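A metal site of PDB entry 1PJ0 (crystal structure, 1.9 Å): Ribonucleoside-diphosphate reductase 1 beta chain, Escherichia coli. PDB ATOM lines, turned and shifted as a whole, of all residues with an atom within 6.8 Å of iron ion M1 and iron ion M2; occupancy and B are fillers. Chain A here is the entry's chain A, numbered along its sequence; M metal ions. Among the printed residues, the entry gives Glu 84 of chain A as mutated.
OE2 of Glu 204 is in hydrogen-bond range of NE2 of Gln 87, at 2.8 Å. A ring nitrogen (ND1) of His 241 lies close to the indole nitrogen (NE1) of Trp 111. The side-chain carboxylate (OE2) of Glu 204 is in hydrogen-bond range of the indole nitrogen (NE1) of Trp 111. The side-chain hydroxyl of Ser 119 is in hydrogen-bond range of the backbone carbonyl oxygen of Glu 115. The backbone carbonyl oxygen (O) of Glu 84 lies close to the side-chain hydroxyl (OG) of Ser 119 (3.5 Å). A ring nitrogen (NE2) of His 118 lies close to the backbone carbonyl oxygen of Ser 114 (3.3 Å). NE2 of His 241 is in hydrogen-bond range of OG of Ser 114 (2.8 Å). The indole nitrogen of Trp 111 lies close to the side-chain carboxylate of Glu 115 (3.2 Å).
Trp 111 touches iron ion M1. Phe 208 touches iron ion M1. The nearest printed residue that does not touch iron ion M1 is His 118 (5.1 Å).
Merely in contact with iron ion M2: Phe 208. Five residues have an atom within 4 Å of iron ion M2: Glu 84, Glu 115, His 118, Phe 208 and Glu 238. The nearest printed residue that does not touch iron ion M2 is Ile 234 (4.2 Å).
OE1 of Glu 238 is bound to iron ion M1. OE2 of Glu 115 is bound to iron ion M1 (1.9 Å). The side-chain carboxylate (OE1) of Glu 204 binds iron ion M1, 2.0 Å away. ND1 of His 241 is bound to iron ion M1 (2.1 Å). Iron ion M1 has four donor atoms within binding distance. Slightly farther from iron ion M1 lies the side-chain carboxylate (OE2) of Glu 204 (2.8 Å).
Iron ion M2 is bound by OE2 of Glu 238 (2.0 Å), ND1 of His 118 (2.1 Å), OE1 of Glu 115 (2.1 Å), OE1 of Glu 84 (2.2 Å) and OE2 of Glu 84 (2.3 Å). Iron ion M2 has five donor atoms within binding distance.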
ATOM      1  N   GLN A  80      -5.361  20.004  -6.155  1.00  0.00           N
ATOM      2  CA  GLN A  80      -5.708  19.092  -7.245  1.00  0.00           C
ATOM      3  C   GLN A  80      -7.176  19.337  -7.643  1.00  0.00           C
ATOM      4  O   GLN A  80      -7.514  19.392  -8.842  1.00  0.00           O
ATOM      5  CB  GLN A  80      -5.532  17.627  -6.798  1.00  0.00           C
ATOM      6  CG  GLN A  80      -4.107  17.253  -6.331  1.00  0.00           C
ATOM      7  CD  GLN A  80      -4.023  15.856  -5.712  1.00  0.00           C
ATOM      8  OE1 GLN A  80      -4.868  15.467  -4.909  1.00  0.00           O
ATOM      9  NE2 GLN A  80      -2.980  15.102  -6.078  1.00  0.00           N
ATOM     10  N   LEU A  83      -7.338  22.508  -9.770  1.00  0.00           N
ATOM     11  CA  LEU A  83      -6.855  22.282 -11.123  1.00  0.00           C
ATOM     12  C   LEU A  83      -7.839  21.484 -11.978  1.00  0.00           C
ATOM     13  O   LEU A  83      -8.026  21.798 -13.151  1.00  0.00           O
ATOM     14  CB  LEU A  83      -5.510  21.550 -11.089  1.00  0.00           C
ATOM     15  CG  LEU A  83      -4.289  22.275 -10.510  1.00  0.00           C
ATOM     16  CD1 LEU A  83      -3.053  21.405 -10.749  1.00  0.00           C
ATOM     17  CD2 LEU A  83      -4.103  23.624 -11.177  1.00  0.00           C
ATOM     18  N   GLU A  84      -8.472  20.466 -11.393  1.00  0.00           N
ATOM     19  CA  GLU A  84      -9.427  19.649 -12.126  1.00  0.00           C
ATOM     20  C   GLU A  84     -10.671  20.443 -12.483  1.00  0.00           C
ATOM     21  O   GLU A  84     -11.246  20.263 -13.566  1.00  0.00           O
ATOM     22  CB  GLU A  84      -9.826  18.402 -11.310  1.00  0.00           C
ATOM     23  CG  GLU A  84      -8.673  17.458 -11.001  1.00  0.00           C
ATOM     24  CD  GLU A  84      -8.076  16.791 -12.244  1.00  0.00           C
ATOM     25  OE1 GLU A  84      -7.196  15.928 -12.085  1.00  0.00           O
ATOM     26  OE2 GLU A  84      -8.479  17.131 -13.375  1.00  0.00           O
ATOM     27  N   GLN A  87      -9.622  22.505 -15.411  1.00  0.00           N
ATOM     28  CA  GLN A  87      -9.384  21.647 -16.571  1.00  0.00           C
ATOM     29  C   GLN A  87     -10.609  20.917 -17.089  1.00  0.00           C
ATOM     30  O   GLN A  87     -10.608  20.423 -18.209  1.00  0.00           O
ATOM     31  CB  GLN A  87      -8.284  20.639 -16.258  1.00  0.00           C
ATOM     32  CG  GLN A  87      -6.896  21.261 -16.174  1.00  0.00           C
ATOM     33  CD  GLN A  87      -6.576  22.122 -17.381  1.00  0.00           C
ATOM     34  OE1 GLN A  87      -6.891  23.313 -17.414  1.00  0.00           O
ATOM     35  NE2 GLN A  87      -5.967  21.528 -18.390  1.00  0.00           N
ATOM     36  N   TRP A 111     -10.664  14.662 -23.484  1.00  0.00           N
ATOM     37  CA  TRP A 111      -9.687  15.061 -22.480  1.00  0.00           C
ATOM     38  C   TRP A 111     -10.425  15.840 -21.381  1.00  0.00           C
ATOM     39  O   TRP A 111     -10.324  15.505 -20.191  1.00  0.00           O
ATOM     40  CB  TRP A 111      -8.611  15.898 -23.189  1.00  0.00           C
ATOM     41  CG  TRP A 111      -7.743  16.789 -22.346  1.00  0.00           C
ATOM     42  CD1 TRP A 111      -7.485  16.672 -21.014  1.00  0.00           C
ATOM     43  CD2 TRP A 111      -6.981  17.904 -22.819  1.00  0.00           C
ATOM     44  NE1 TRP A 111      -6.606  17.662 -20.623  1.00  0.00           N
ATOM     45  CE2 TRP A 111      -6.280  18.429 -21.716  1.00  0.00           C
ATOM     46  CE3 TRP A 111      -6.826  18.520 -24.067  1.00  0.00           C
ATOM     47  CZ2 TRP A 111      -5.432  19.540 -21.821  1.00  0.00           C
ATOM     48  CZ3 TRP A 111      -5.981  19.618 -24.184  1.00  0.00           C
ATOM     49  CH2 TRP A 111      -5.298  20.117 -23.055  1.00  0.00           C
ATOM     50  N   SER A 114     -12.666  13.648 -19.161  1.00  0.00           N
ATOM     51  CA  SER A 114     -11.946  12.836 -18.185  1.00  0.00           C
ATOM     52  C   SER A 114     -11.553  13.692 -16.978  1.00  0.00           C
ATOM     53  O   SER A 114     -11.465  13.181 -15.867  1.00  0.00           O
ATOM     54  CB  SER A 114     -10.711  12.177 -18.806  1.00  0.00           C
ATOM     55  OG  SER A 114      -9.674  13.104 -19.016  1.00  0.00           O
ATOM     56  N   GLU A 115     -11.329  14.985 -17.188  1.00  0.00           N
ATOM     57  CA  GLU A 115     -10.963  15.854 -16.062  1.00  0.00           C
ATOM     58  C   GLU A 115     -12.158  15.990 -15.113  1.00  0.00           C
ATOM     59  O   GLU A 115     -11.978  16.079 -13.895  1.00  0.00           O
ATOM     60  CB  GLU A 115     -10.506  17.244 -16.557  1.00  0.00           C
ATOM     61  CG  GLU A 115      -9.348  17.216 -17.577  1.00  0.00           C
ATOM     62  CD  GLU A 115      -7.993  16.793 -16.996  1.00  0.00           C
ATOM     63  OE1 GLU A 115      -7.957  15.898 -16.144  1.00  0.00           O
ATOM     64  OE2 GLU A 115      -6.959  17.350 -17.420  1.00  0.00           O
ATOM     65  N   THR A 116     -13.388  16.004 -15.633  1.00  0.00           N
ATOM     66  CA  THR A 116     -14.540  16.107 -14.745  1.00  0.00           C
ATOM     67  C   THR A 116     -14.706  14.811 -13.957  1.00  0.00           C
ATOM     68  O   THR A 116     -15.267  14.816 -12.859  1.00  0.00           O
ATOM     69  CB  THR A 116     -15.883  16.432 -15.491  1.00  0.00           C
ATOM     70  OG1 THR A 116     -16.319  15.291 -16.245  1.00  0.00           O
ATOM     71  CG2 THR A 116     -15.689  17.628 -16.418  1.00  0.00           C
ATOM     72  N   HIS A 118     -12.184  13.221 -12.858  1.00  0.00           N
ATOM     73  CA  HIS A 118     -11.196  13.403 -11.801  1.00  0.00           C
ATOM     74  C   HIS A 118     -11.797  14.290 -10.714  1.00  0.00           C
ATOM     75  O   HIS A 118     -11.572  14.081  -9.518  1.00  0.00           O
ATOM     76  CB  HIS A 118      -9.936  14.036 -12.378  1.00  0.00           C
ATOM     77  CG  HIS A 118      -9.295  13.199 -13.443  1.00  0.00           C
ATOM     78  ND1 HIS A 118      -8.205  13.619 -14.165  1.00  0.00           N
ATOM     79  CD2 HIS A 118      -9.592  11.960 -13.909  1.00  0.00           C
ATOM     80  CE1 HIS A 118      -7.860  12.683 -15.035  1.00  0.00           C
ATOM     81  NE2 HIS A 118      -8.689  11.660 -14.892  1.00  0.00           N
ATOM     82  N   SER A 119     -12.573  15.289 -11.121  1.00  0.00           N
ATOM     83  CA  SER A 119     -13.220  16.178 -10.151  1.00  0.00           C
ATOM     84  C   SER A 119     -14.192  15.375  -9.306  1.00  0.00           C
ATOM     85  O   SER A 119     -14.243  15.524  -8.081  1.00  0.00           O
ATOM     86  CB  SER A 119     -13.986  17.290 -10.876  1.00  0.00           C
ATOM     87  OG  SER A 119     -13.091  18.207 -11.470  1.00  0.00           O
ATOM     88  N   TYR A 122     -12.425  13.457  -6.649  1.00  0.00           N
ATOM     89  CA  TYR A 122     -12.045  14.229  -5.469  1.00  0.00           C
ATOM     90  C   TYR A 122     -13.234  14.527  -4.547  1.00  0.00           C
ATOM     91  O   TYR A 122     -13.066  14.653  -3.342  1.00  0.00           O
ATOM     92  CB  TYR A 122     -11.317  15.510  -5.877  1.00  0.00           C
ATOM     93  CG  TYR A 122      -9.924  15.236  -6.417  1.00  0.00           C
ATOM     94  CD1 TYR A 122      -9.000  14.539  -5.651  1.00  0.00           C
ATOM     95  CD2 TYR A 122      -9.527  15.690  -7.670  1.00  0.00           C
ATOM     96  CE1 TYR A 122      -7.714  14.283  -6.117  1.00  0.00           C
ATOM     97  CE2 TYR A 122      -8.240  15.444  -8.157  1.00  0.00           C
ATOM     98  CZ  TYR A 122      -7.336  14.742  -7.355  1.00  0.00           C
ATOM     99  OH  TYR A 122      -6.046  14.481  -7.789  1.00  0.00           O
ATOM    100  N   GLU A 204      -0.473  20.243 -16.912  1.00  0.00           N
ATOM    101  CA  GLU A 204      -0.664  18.802 -17.017  1.00  0.00           C
ATOM    102  C   GLU A 204       0.582  17.976 -16.660  1.00  0.00           C
ATOM    103  O   GLU A 204       0.484  16.956 -15.973  1.00  0.00           O
ATOM    104  CB  GLU A 204      -1.076  18.425 -18.441  1.00  0.00           C
ATOM    105  CG  GLU A 204      -2.378  19.036 -18.984  1.00  0.00           C
ATOM    106  CD  GLU A 204      -3.627  18.346 -18.478  1.00  0.00           C
ATOM    107  OE1 GLU A 204      -3.537  17.180 -18.062  1.00  0.00           O
ATOM    108  OE2 GLU A 204      -4.711  18.980 -18.490  1.00  0.00           O
ATOM    109  N   PHE A 208       0.419  18.762 -11.837  1.00  0.00           N
ATOM    110  CA  PHE A 208      -0.298  17.552 -11.414  1.00  0.00           C
ATOM    111  C   PHE A 208       0.655  16.500 -10.842  1.00  0.00           C
ATOM    112  O   PHE A 208       0.319  15.814  -9.875  1.00  0.00           O
ATOM    113  CB  PHE A 208      -1.063  16.907 -12.589  1.00  0.00           C
ATOM    114  CG  PHE A 208      -2.427  17.491 -12.838  1.00  0.00           C
ATOM    115  CD1 PHE A 208      -3.331  17.699 -11.794  1.00  0.00           C
ATOM    116  CD2 PHE A 208      -2.852  17.792 -14.142  1.00  0.00           C
ATOM    117  CE1 PHE A 208      -4.613  18.187 -12.031  1.00  0.00           C
ATOM    118  CE2 PHE A 208      -4.131  18.280 -14.389  1.00  0.00           C
ATOM    119  CZ  PHE A 208      -5.016  18.478 -13.319  1.00  0.00           C
ATOM    120  N   PHE A 212       0.905  14.590  -7.216  1.00  0.00           N
ATOM    121  CA  PHE A 212       0.838  13.134  -7.109  1.00  0.00           C
ATOM    122  C   PHE A 212       1.889  12.641  -6.116  1.00  0.00           C
ATOM    123  O   PHE A 212       1.647  11.713  -5.345  1.00  0.00           O
ATOM    124  CB  PHE A 212       1.076  12.453  -8.454  1.00  0.00           C
ATOM    125  CG  PHE A 212       0.028  12.758  -9.490  1.00  0.00           C
ATOM    126  CD1 PHE A 212      -1.275  13.063  -9.111  1.00  0.00           C
ATOM    127  CD2 PHE A 212       0.344  12.714 -10.846  1.00  0.00           C
ATOM    128  CE1 PHE A 212      -2.248  13.330 -10.074  1.00  0.00           C
ATOM    129  CE2 PHE A 212      -0.614  12.976 -11.815  1.00  0.00           C
ATOM    130  CZ  PHE A 212      -1.920  13.280 -11.427  1.00  0.00           C
ATOM    131  N   ILE A 234      -5.968   8.557 -12.008  1.00  0.00           N
ATOM    132  CA  ILE A 234      -5.902   9.918 -12.512  1.00  0.00           C
ATOM    133  C   ILE A 234      -4.593  10.154 -13.246  1.00  0.00           C
ATOM    134  O   ILE A 234      -4.586  10.704 -14.350  1.00  0.00           O
ATOM    135  CB  ILE A 234      -6.034  10.948 -11.350  1.00  0.00           C
ATOM    136  CG1 ILE A 234      -7.478  10.980 -10.859  1.00  0.00           C
ATOM    137  CG2 ILE A 234      -5.580  12.351 -11.814  1.00  0.00           C
ATOM    138  CD1 ILE A 234      -7.717  11.944  -9.697  1.00  0.00           C
ATOM    139  N   ASP A 237      -4.387   8.982 -16.719  1.00  0.00           N
ATOM    140  CA  ASP A 237      -5.032   9.905 -17.652  1.00  0.00           C
ATOM    141  C   ASP A 237      -4.161  11.123 -17.958  1.00  0.00           C
ATOM    142  O   ASP A 237      -4.016  11.496 -19.118  1.00  0.00           O
ATOM    143  CB  ASP A 237      -6.373  10.407 -17.094  1.00  0.00           C
ATOM    144  CG  ASP A 237      -7.434   9.334 -17.049  1.00  0.00           C
ATOM    145  OD1 ASP A 237      -7.259   8.277 -17.700  1.00  0.00           O
ATOM    146  OD2 ASP A 237      -8.450   9.548 -16.360  1.00  0.00           O
ATOM    147  N   GLU A 238      -3.586  11.731 -16.931  1.00  0.00           N
ATOM    148  CA  GLU A 238      -2.735  12.898 -17.129  1.00  0.00           C
ATOM    149  C   GLU A 238      -1.564  12.580 -18.077  1.00  0.00           C
ATOM    150  O   GLU A 238      -1.096  13.452 -18.805  1.00  0.00           O
ATOM    151  CB  GLU A 238      -2.186  13.440 -15.799  1.00  0.00           C
ATOM    152  CG  GLU A 238      -3.250  13.842 -14.767  1.00  0.00           C
ATOM    153  CD  GLU A 238      -4.312  14.775 -15.330  1.00  0.00           C
ATOM    154  OE1 GLU A 238      -4.089  15.395 -16.392  1.00  0.00           O
ATOM    155  OE2 GLU A 238      -5.393  14.891 -14.703  1.00  0.00           O
ATOM    156  N   ALA A 239      -1.106  11.326 -18.055  1.00  0.00           N
ATOM    157  CA  ALA A 239      -0.005  10.921 -18.941  1.00  0.00           C
ATOM    158  C   ALA A 239      -0.464  11.041 -20.403  1.00  0.00           C
ATOM    159  O   ALA A 239       0.322  11.431 -21.275  1.00  0.00           O
ATOM    160  CB  ALA A 239       0.401   9.482 -18.625  1.00  0.00           C
ATOM    161  N   HIS A 241      -2.930  13.064 -21.407  1.00  0.00           N
ATOM    162  CA  HIS A 241      -3.169  14.484 -21.613  1.00  0.00           C
ATOM    163  C   HIS A 241      -1.907  15.258 -21.979  1.00  0.00           C
ATOM    164  O   HIS A 241      -1.914  16.059 -22.907  1.00  0.00           O
ATOM    165  CB  HIS A 241      -3.806  15.091 -20.373  1.00  0.00           C
ATOM    166  CG  HIS A 241      -5.117  14.459 -20.009  1.00  0.00           C
ATOM    167  ND1 HIS A 241      -5.796  14.770 -18.847  1.00  0.00           N
ATOM    168  CD2 HIS A 241      -5.871  13.527 -20.644  1.00  0.00           C
ATOM    169  CE1 HIS A 241      -6.909  14.046 -18.792  1.00  0.00           C
ATOM    170  NE2 HIS A 241      -6.976  13.291 -19.872  1.00  0.00           N
ATOM    171  N   LEU A 242      -0.815  15.014 -21.263  1.00  0.00           N
ATOM    172  CA  LEU A 242       0.413  15.726 -21.577  1.00  0.00           C
ATOM    173  C   LEU A 242       1.033  15.152 -22.842  1.00  0.00           C
ATOM    174  O   LEU A 242       1.803  15.825 -23.538  1.00  0.00           O
ATOM    175  CB  LEU A 242       1.387  15.666 -20.382  1.00  0.00           C
ATOM    176  CG  LEU A 242       2.037  14.344 -19.994  1.00  0.00           C
ATOM    177  CD1 LEU A 242       3.265  14.109 -20.872  1.00  0.00           C
ATOM    178  CD2 LEU A 242       2.474  14.399 -18.526  1.00  0.00           C
HETATM  179 FE    FE M   1      -5.290  16.352 -17.557  1.00  0.00          FE
HETATM  180 FE    FE M   2      -7.190  15.465 -14.192  1.00  0.00          FE
